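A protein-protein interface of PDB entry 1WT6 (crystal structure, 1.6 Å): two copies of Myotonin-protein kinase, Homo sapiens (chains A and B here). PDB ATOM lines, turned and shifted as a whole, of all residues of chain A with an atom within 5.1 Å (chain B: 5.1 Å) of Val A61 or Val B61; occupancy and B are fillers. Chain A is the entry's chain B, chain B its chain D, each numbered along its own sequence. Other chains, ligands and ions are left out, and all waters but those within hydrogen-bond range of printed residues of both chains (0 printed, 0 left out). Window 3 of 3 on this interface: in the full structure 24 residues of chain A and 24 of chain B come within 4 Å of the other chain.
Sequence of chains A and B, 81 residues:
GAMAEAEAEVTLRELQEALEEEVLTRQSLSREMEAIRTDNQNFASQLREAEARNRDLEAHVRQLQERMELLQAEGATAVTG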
ATOM      1  N   LEU A  57       4.484  18.712  -4.255  1.00  0.00           N
ATOM      2  CA  LEU A  57       3.786  19.657  -5.126  1.00  0.00           C
ATOM      3  C   LEU A  57       3.812  21.091  -4.546  1.00  0.00           C
ATOM      4  O   LEU A  57       3.985  22.047  -5.292  1.00  0.00           O
ATOM      5  CB  LEU A  57       2.357  19.169  -5.349  1.00  0.00           C
ATOM      6  CG  LEU A  57       1.678  19.858  -6.536  1.00  0.00           C
ATOM      7  CD1 LEU A  57       2.499  19.658  -7.871  1.00  0.00           C
ATOM      8  CD2 LEU A  57       0.268  19.219  -6.582  1.00  0.00           C
ATOM      9  N   GLU A  58       3.667  21.217  -3.237  1.00  0.00           N
ATOM     10  CA  GLU A  58       3.818  22.509  -2.581  1.00  0.00           C
ATOM     11  C   GLU A  58       5.178  23.170  -2.909  1.00  0.00           C
ATOM     12  O   GLU A  58       5.234  24.356  -3.230  1.00  0.00           O
ATOM     13  CB  GLU A  58       3.668  22.381  -1.089  1.00  0.00           C
ATOM     14  CG  GLU A  58       2.310  22.055  -0.616  1.00  0.00           C
ATOM     15  CD  GLU A  58       2.276  21.905   0.941  1.00  0.00           C
ATOM     16  OE1 GLU A  58       3.406  21.887   1.540  1.00  0.00           O
ATOM     17  OE2 GLU A  58       1.159  21.760   1.561  1.00  0.00           O
ATOM     18  N   ALA A  59       6.251  22.363  -2.833  1.00  0.00           N
ATOM     19  CA  ALA A  59       7.596  22.884  -3.133  1.00  0.00           C
ATOM     20  C   ALA A  59       7.665  23.345  -4.583  1.00  0.00           C
ATOM     21  O   ALA A  59       8.287  24.392  -4.890  1.00  0.00           O
ATOM     22  CB  ALA A  59       8.657  21.828  -2.834  1.00  0.00           C
ATOM     23  N   HIS A  60       7.066  22.573  -5.494  1.00  0.00           N
ATOM     24  CA  HIS A  60       7.129  22.934  -6.908  1.00  0.00           C
ATOM     25  C   HIS A  60       6.385  24.227  -7.166  1.00  0.00           C
ATOM     26  O   HIS A  60       6.877  25.069  -7.915  1.00  0.00           O
ATOM     27  CB  HIS A  60       6.598  21.821  -7.810  1.00  0.00           C
ATOM     28  CG  HIS A  60       7.474  20.599  -7.841  1.00  0.00           C
ATOM     29  ND1 HIS A  60       8.749  20.598  -8.386  1.00  0.00           N
ATOM     30  CD2 HIS A  60       7.257  19.335  -7.385  1.00  0.00           C
ATOM     31  CE1 HIS A  60       9.273  19.383  -8.274  1.00  0.00           C
ATOM     32  NE2 HIS A  60       8.393  18.598  -7.661  1.00  0.00           N
ATOM     33  N   VAL A  61       5.235  24.392  -6.504  1.00  0.00           N
ATOM     34  CA  VAL A  61       4.394  25.563  -6.678  1.00  0.00           C
ATOM     35  C   VAL A  61       5.111  26.792  -6.090  1.00  0.00           C
ATOM     36  O   VAL A  61       5.027  27.861  -6.686  1.00  0.00           O
ATOM     37  CB  VAL A  61       2.997  25.346  -6.063  1.00  0.00           C
ATOM     38  CG1 VAL A  61       2.177  26.661  -5.901  1.00  0.00           C
ATOM     39  CG2 VAL A  61       2.251  24.236  -6.985  1.00  0.00           C
ATOM     40  N   ARG A  62       5.799  26.637  -4.957  1.00  0.00           N
ATOM     41  CA  ARG A  62       6.608  27.744  -4.408  1.00  0.00           C
ATOM     42  C   ARG A  62       7.626  28.205  -5.432  1.00  0.00           C
ATOM     43  O   ARG A  62       7.761  29.411  -5.663  1.00  0.00           O
ATOM     44  CB  ARG A  62       7.279  27.374  -3.058  1.00  0.00           C
ATOM     45  CG  ARG A  62       6.418  27.769  -1.827  1.00  0.00           C
ATOM     46  CD  ARG A  62       7.186  27.683  -0.480  1.00  0.00           C
ATOM     47  NE  ARG A  62       8.214  26.643  -0.495  1.00  0.00           N
ATOM     48  CZ  ARG A  62       8.062  25.393  -0.056  1.00  0.00           C
ATOM     49  NH1 ARG A  62       6.912  24.983   0.475  1.00  0.00           N
ATOM     50  NH2 ARG A  62       9.081  24.544  -0.131  1.00  0.00           N
ATOM     51  N   GLN A  63       8.334  27.267  -6.046  1.00  0.00           N
ATOM     52  CA  GLN A  63       9.294  27.600  -7.109  1.00  0.00           C
ATOM     53  C   GLN A  63       8.673  28.374  -8.264  1.00  0.00           C
ATOM     54  O   GLN A  63       9.312  29.291  -8.817  1.00  0.00           O
ATOM     55  CB  GLN A  63       9.959  26.342  -7.702  1.00  0.00           C
ATOM     56  CG  GLN A  63      11.362  25.979  -7.171  1.00  0.00           C
ATOM     57  CD  GLN A  63      12.334  25.449  -8.274  1.00  0.00           C
ATOM     58  OE1 GLN A  63      12.006  24.500  -9.025  1.00  0.00           O
ATOM     59  NE2 GLN A  63      13.546  26.057  -8.351  1.00  0.00           N
ATOM     60  N   LEU A  64       7.471  27.963  -8.686  1.00  0.00           N
ATOM     61  CA  LEU A  64       6.765  28.656  -9.764  1.00  0.00           C
ATOM     62  C   LEU A  64       6.306  30.035  -9.357  1.00  0.00           C
ATOM     63  O   LEU A  64       6.324  30.955 -10.201  1.00  0.00           O
ATOM     64  CB  LEU A  64       5.550  27.872 -10.231  1.00  0.00           C
ATOM     65  CG  LEU A  64       5.890  26.523 -10.827  1.00  0.00           C
ATOM     66  CD1 LEU A  64       4.563  25.814 -11.125  1.00  0.00           C
ATOM     67  CD2 LEU A  64       6.851  26.584 -12.047  1.00  0.00           C
ATOM     68  N   GLN A  65       5.886  30.185  -8.106  1.00  0.00           N
ATOM     69  CA  GLN A  65       5.462  31.525  -7.579  1.00  0.00           C
ATOM     70  C   GLN A  65       6.638  32.508  -7.585  1.00  0.00           C
ATOM     71  O   GLN A  65       6.501  33.663  -7.952  1.00  0.00           O
ATOM     72  CB  GLN A  65       4.892  31.444  -6.161  1.00  0.00           C
ATOM     73  CG  GLN A  65       3.553  30.690  -6.015  1.00  0.00           C
ATOM     74  CD  GLN A  65       3.111  30.496  -4.549  1.00  0.00           C
ATOM     75  OE1 GLN A  65       3.931  30.237  -3.650  1.00  0.00           O
ATOM     76  NE2 GLN A  65       1.809  30.599  -4.313  1.00  0.00           N
ATOM     77  N   GLU A  66       7.798  31.998  -7.216  1.00  0.00           N
ATOM     78  CA  GLU A  66       9.046  32.771  -7.180  1.00  0.00           C
ATOM     79  C   GLU A  66       9.495  33.137  -8.580  1.00  0.00           C
ATOM     80  O   GLU A  66       9.900  34.285  -8.829  1.00  0.00           O
ATOM     81  CB  GLU A  66      10.124  31.963  -6.451  1.00  0.00           C
ATOM     82  CG  GLU A  66       9.893  31.977  -4.960  1.00  0.00           C
ATOM     83  CD  GLU A  66      10.636  30.904  -4.183  1.00  0.00           C
ATOM     84  OE1 GLU A  66      11.463  30.170  -4.773  1.00  0.00           O
ATOM     85  OE2 GLU A  66      10.377  30.810  -2.958  1.00  0.00           O
ATOM     86  N   LEU B  57      -4.279  18.164  -9.771  1.00  0.00           N
ATOM     87  CA  LEU B  57      -3.467  19.338  -9.472  1.00  0.00           C
ATOM     88  C   LEU B  57      -2.024  19.196 -10.038  1.00  0.00           C
ATOM     89  O   LEU B  57      -1.494  20.125 -10.645  1.00  0.00           O
ATOM     90  CB  LEU B  57      -3.486  19.559  -7.941  1.00  0.00           C
ATOM     91  CG  LEU B  57      -2.982  20.971  -7.594  1.00  0.00           C
ATOM     92  CD1 LEU B  57      -3.815  22.112  -8.257  1.00  0.00           C
ATOM     93  CD2 LEU B  57      -3.150  21.108  -6.061  1.00  0.00           C
ATOM     94  N   GLU B  58      -1.429  18.005  -9.943  1.00  0.00           N
ATOM     95  CA  GLU B  58      -0.082  17.808 -10.488  1.00  0.00           C
ATOM     96  C   GLU B  58      -0.058  18.119 -11.995  1.00  0.00           C
ATOM     97  O   GLU B  58       0.845  18.766 -12.545  1.00  0.00           O
ATOM     98  CB  GLU B  58       0.378  16.389 -10.245  1.00  0.00           C
ATOM     99  CG  GLU B  58       0.750  16.095  -8.802  1.00  0.00           C
ATOM    100  CD  GLU B  58       1.089  14.625  -8.570  1.00  0.00           C
ATOM    101  OE1 GLU B  58       0.762  13.729  -9.416  1.00  0.00           O
ATOM    102  OE2 GLU B  58       1.661  14.328  -7.509  1.00  0.00           O
ATOM    103  N   ALA B  59      -1.111  17.649 -12.668  1.00  0.00           N
ATOM    104  CA  ALA B  59      -1.255  17.917 -14.126  1.00  0.00           C
ATOM    105  C   ALA B  59      -1.347  19.428 -14.429  1.00  0.00           C
ATOM    106  O   ALA B  59      -0.728  19.968 -15.367  1.00  0.00           O
ATOM    107  CB  ALA B  59      -2.507  17.164 -14.662  1.00  0.00           C
ATOM    108  N   HIS B  60      -2.109  20.160 -13.618  1.00  0.00           N
ATOM    109  CA  HIS B  60      -2.229  21.578 -13.805  1.00  0.00           C
ATOM    110  C   HIS B  60      -0.911  22.333 -13.546  1.00  0.00           C
ATOM    111  O   HIS B  60      -0.592  23.291 -14.266  1.00  0.00           O
ATOM    112  CB  HIS B  60      -3.363  22.103 -12.961  1.00  0.00           C
ATOM    113  CG  HIS B  60      -4.690  21.784 -13.561  1.00  0.00           C
ATOM    114  ND1 HIS B  60      -5.098  22.323 -14.764  1.00  0.00           N
ATOM    115  CD2 HIS B  60      -5.682  20.942 -13.169  1.00  0.00           C
ATOM    116  CE1 HIS B  60      -6.293  21.847 -15.073  1.00  0.00           C
ATOM    117  NE2 HIS B  60      -6.670  21.014 -14.122  1.00  0.00           N
ATOM    118  N   VAL B  61      -0.170  21.880 -12.534  1.00  0.00           N
ATOM    119  CA  VAL B  61       1.138  22.445 -12.234  1.00  0.00           C
ATOM    120  C   VAL B  61       2.095  22.253 -13.376  1.00  0.00           C
ATOM    121  O   VAL B  61       2.777  23.194 -13.776  1.00  0.00           O
ATOM    122  CB  VAL B  61       1.707  21.950 -10.926  1.00  0.00           C
ATOM    123  CG1 VAL B  61       3.145  22.447 -10.776  1.00  0.00           C
ATOM    124  CG2 VAL B  61       0.746  22.406  -9.761  1.00  0.00           C
ATOM    125  N   ARG B  62       2.101  21.053 -13.935  1.00  0.00           N
ATOM    126  CA  ARG B  62       2.913  20.806 -15.145  1.00  0.00           C
ATOM    127  C   ARG B  62       2.588  21.739 -16.286  1.00  0.00           C
ATOM    128  O   ARG B  62       3.509  22.293 -16.948  1.00  0.00           O
ATOM    129  CB  ARG B  62       2.814  19.349 -15.572  1.00  0.00           C
ATOM    130  CG  ARG B  62       3.497  18.428 -14.599  1.00  0.00           C
ATOM    131  CD  ARG B  62       3.748  16.990 -15.191  1.00  0.00           C
ATOM    132  NE  ARG B  62       2.467  16.334 -15.466  1.00  0.00           N
ATOM    133  CZ  ARG B  62       1.878  15.466 -14.647  1.00  0.00           C
ATOM    134  NH1 ARG B  62       2.487  15.098 -13.531  1.00  0.00           N
ATOM    135  NH2 ARG B  62       0.699  14.942 -14.968  1.00  0.00           N
ATOM    136  N   GLN B  63       1.304  21.935 -16.552  1.00  0.00           N
ATOM    137  CA  GLN B  63       0.912  22.852 -17.624  1.00  0.00           C
ATOM    138  C   GLN B  63       1.380  24.286 -17.336  1.00  0.00           C
ATOM    139  O   GLN B  63       1.802  24.994 -18.233  1.00  0.00           O
ATOM    140  CB  GLN B  63      -0.602  22.839 -17.783  1.00  0.00           C
ATOM    141  CG  GLN B  63      -1.093  23.775 -18.850  1.00  0.00           C
ATOM    142  CD  GLN B  63      -2.262  23.191 -19.613  1.00  0.00           C
ATOM    143  OE1 GLN B  63      -3.106  22.495 -19.043  1.00  0.00           O
ATOM    144  NE2 GLN B  63      -2.315  23.466 -20.918  1.00  0.00           N
ATOM    145  N   LEU B  64       1.288  24.724 -16.092  1.00  0.00           N
ATOM    146  CA  LEU B  64       1.811  26.058 -15.708  1.00  0.00           C
ATOM    147  C   LEU B  64       3.313  26.152 -15.922  1.00  0.00           C
ATOM    148  O   LEU B  64       3.793  27.160 -16.417  1.00  0.00           O
ATOM    149  CB  LEU B  64       1.518  26.431 -14.237  1.00  0.00           C
ATOM    150  CG  LEU B  64       0.074  26.783 -13.950  1.00  0.00           C
ATOM    151  CD1 LEU B  64       0.039  27.148 -12.447  1.00  0.00           C
ATOM    152  CD2 LEU B  64      -0.419  27.996 -14.757  1.00  0.00           C
ATOM    153  N   GLN B  65       4.039  25.114 -15.536  1.00  0.00           N
ATOM    154  CA  GLN B  65       5.501  25.116 -15.650  1.00  0.00           C
ATOM    155  C   GLN B  65       5.851  25.280 -17.132  1.00  0.00           C
ATOM    156  O   GLN B  65       6.742  26.063 -17.509  1.00  0.00           O
ATOM    157  CB  GLN B  65       6.112  23.826 -15.089  1.00  0.00           C
ATOM    158  CG  GLN B  65       5.980  23.649 -13.552  1.00  0.00           C
ATOM    159  CD  GLN B  65       6.397  22.259 -13.038  1.00  0.00           C
ATOM    160  OE1 GLN B  65       6.309  21.260 -13.772  1.00  0.00           O
ATOM    161  NE2 GLN B  65       6.850  22.193 -11.763  1.00  0.00           N
ATOM    162  N   GLU B  66       5.108  24.580 -17.974  1.00  0.00           N
ATOM    163  CA  GLU B  66       5.426  24.564 -19.408  1.00  0.00           C
ATOM    164  C   GLU B  66       5.107  25.908 -20.047  1.00  0.00           C
ATOM    165  O   GLU B  66       5.897  26.407 -20.866  1.00  0.00           O
ATOM    166  CB  GLU B  66       4.712  23.404 -20.085  1.00  0.00           C
ATOM    167  CG  GLU B  66       5.114  22.084 -19.431  1.00  0.00           C
ATOM    168  CD  GLU B  66       4.159  20.930 -19.700  1.00  0.00           C
ATOM    169  OE1 GLU B  66       3.051  21.166 -20.243  1.00  0.00           O
ATOM    170  OE2 GLU B  66       4.535  19.782 -19.352  1.00  0.00           O
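Among the printed residues, pairs that only touch across the chains: Leu A57 with Leu B57, Leu A57 with Glu B58, Leu A57 with Val B61, His A60 with Gln B65, Val A61 with Val B61, Leu A64 with Val B61 and Leu A64 with Gln B65.
Hydrophobic or aromatic side chains of chain B within 4 Å of the printed part of chain A: Leu B57 and Val B61. Along chain A the printed residues that touch a printed residue of chain B span positions 57 to 64. Among the printed residues, 7 pairs touch across the chains.
Of the printed residues of chain B, His A60 touches Gln B65 (3.98 Å). Of chain B, only Val B61 (3.6 Å) comes within 4 Å of Val A61. Printed residues of chain B within 4 Å of Leu A64: Val B61 (3.7 Å) and Gln B65 (3.4 Å). Of the printed residues of chain A, Leu B57 touches Leu A57 (3.8 Å). Of the printed residues of chain A, Glu B58 touches Leu A57 (3.9 Å). Of the printed residues of chain A, Val B61 touches Leu A57, Val A61 and Leu A64. Arg B62 touches none of the printed residues of chain A. The nearest printed residue of chain B that does not touch Val A61 is Gln B65 (5.9 Å). The nearest printed residue of chain B that does not touch His A60 is Val B61 (4.6 Å).
Leu B57 touches its own counterpart, Leu A57. His A60 touches Gln B65, but with the chains exchanged Gln A65 does not touch His B60 (11.3 Å). Val A61 touches its own counterpart, Val B61. Leu A64 touches Gln B65, but with the chains exchanged Gln A65 does not touch Leu B64 (7.9 Å). Of the 7 pairs that touch across the chains among the printed residues, 2 have their exchanged pair printed and touching as well.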
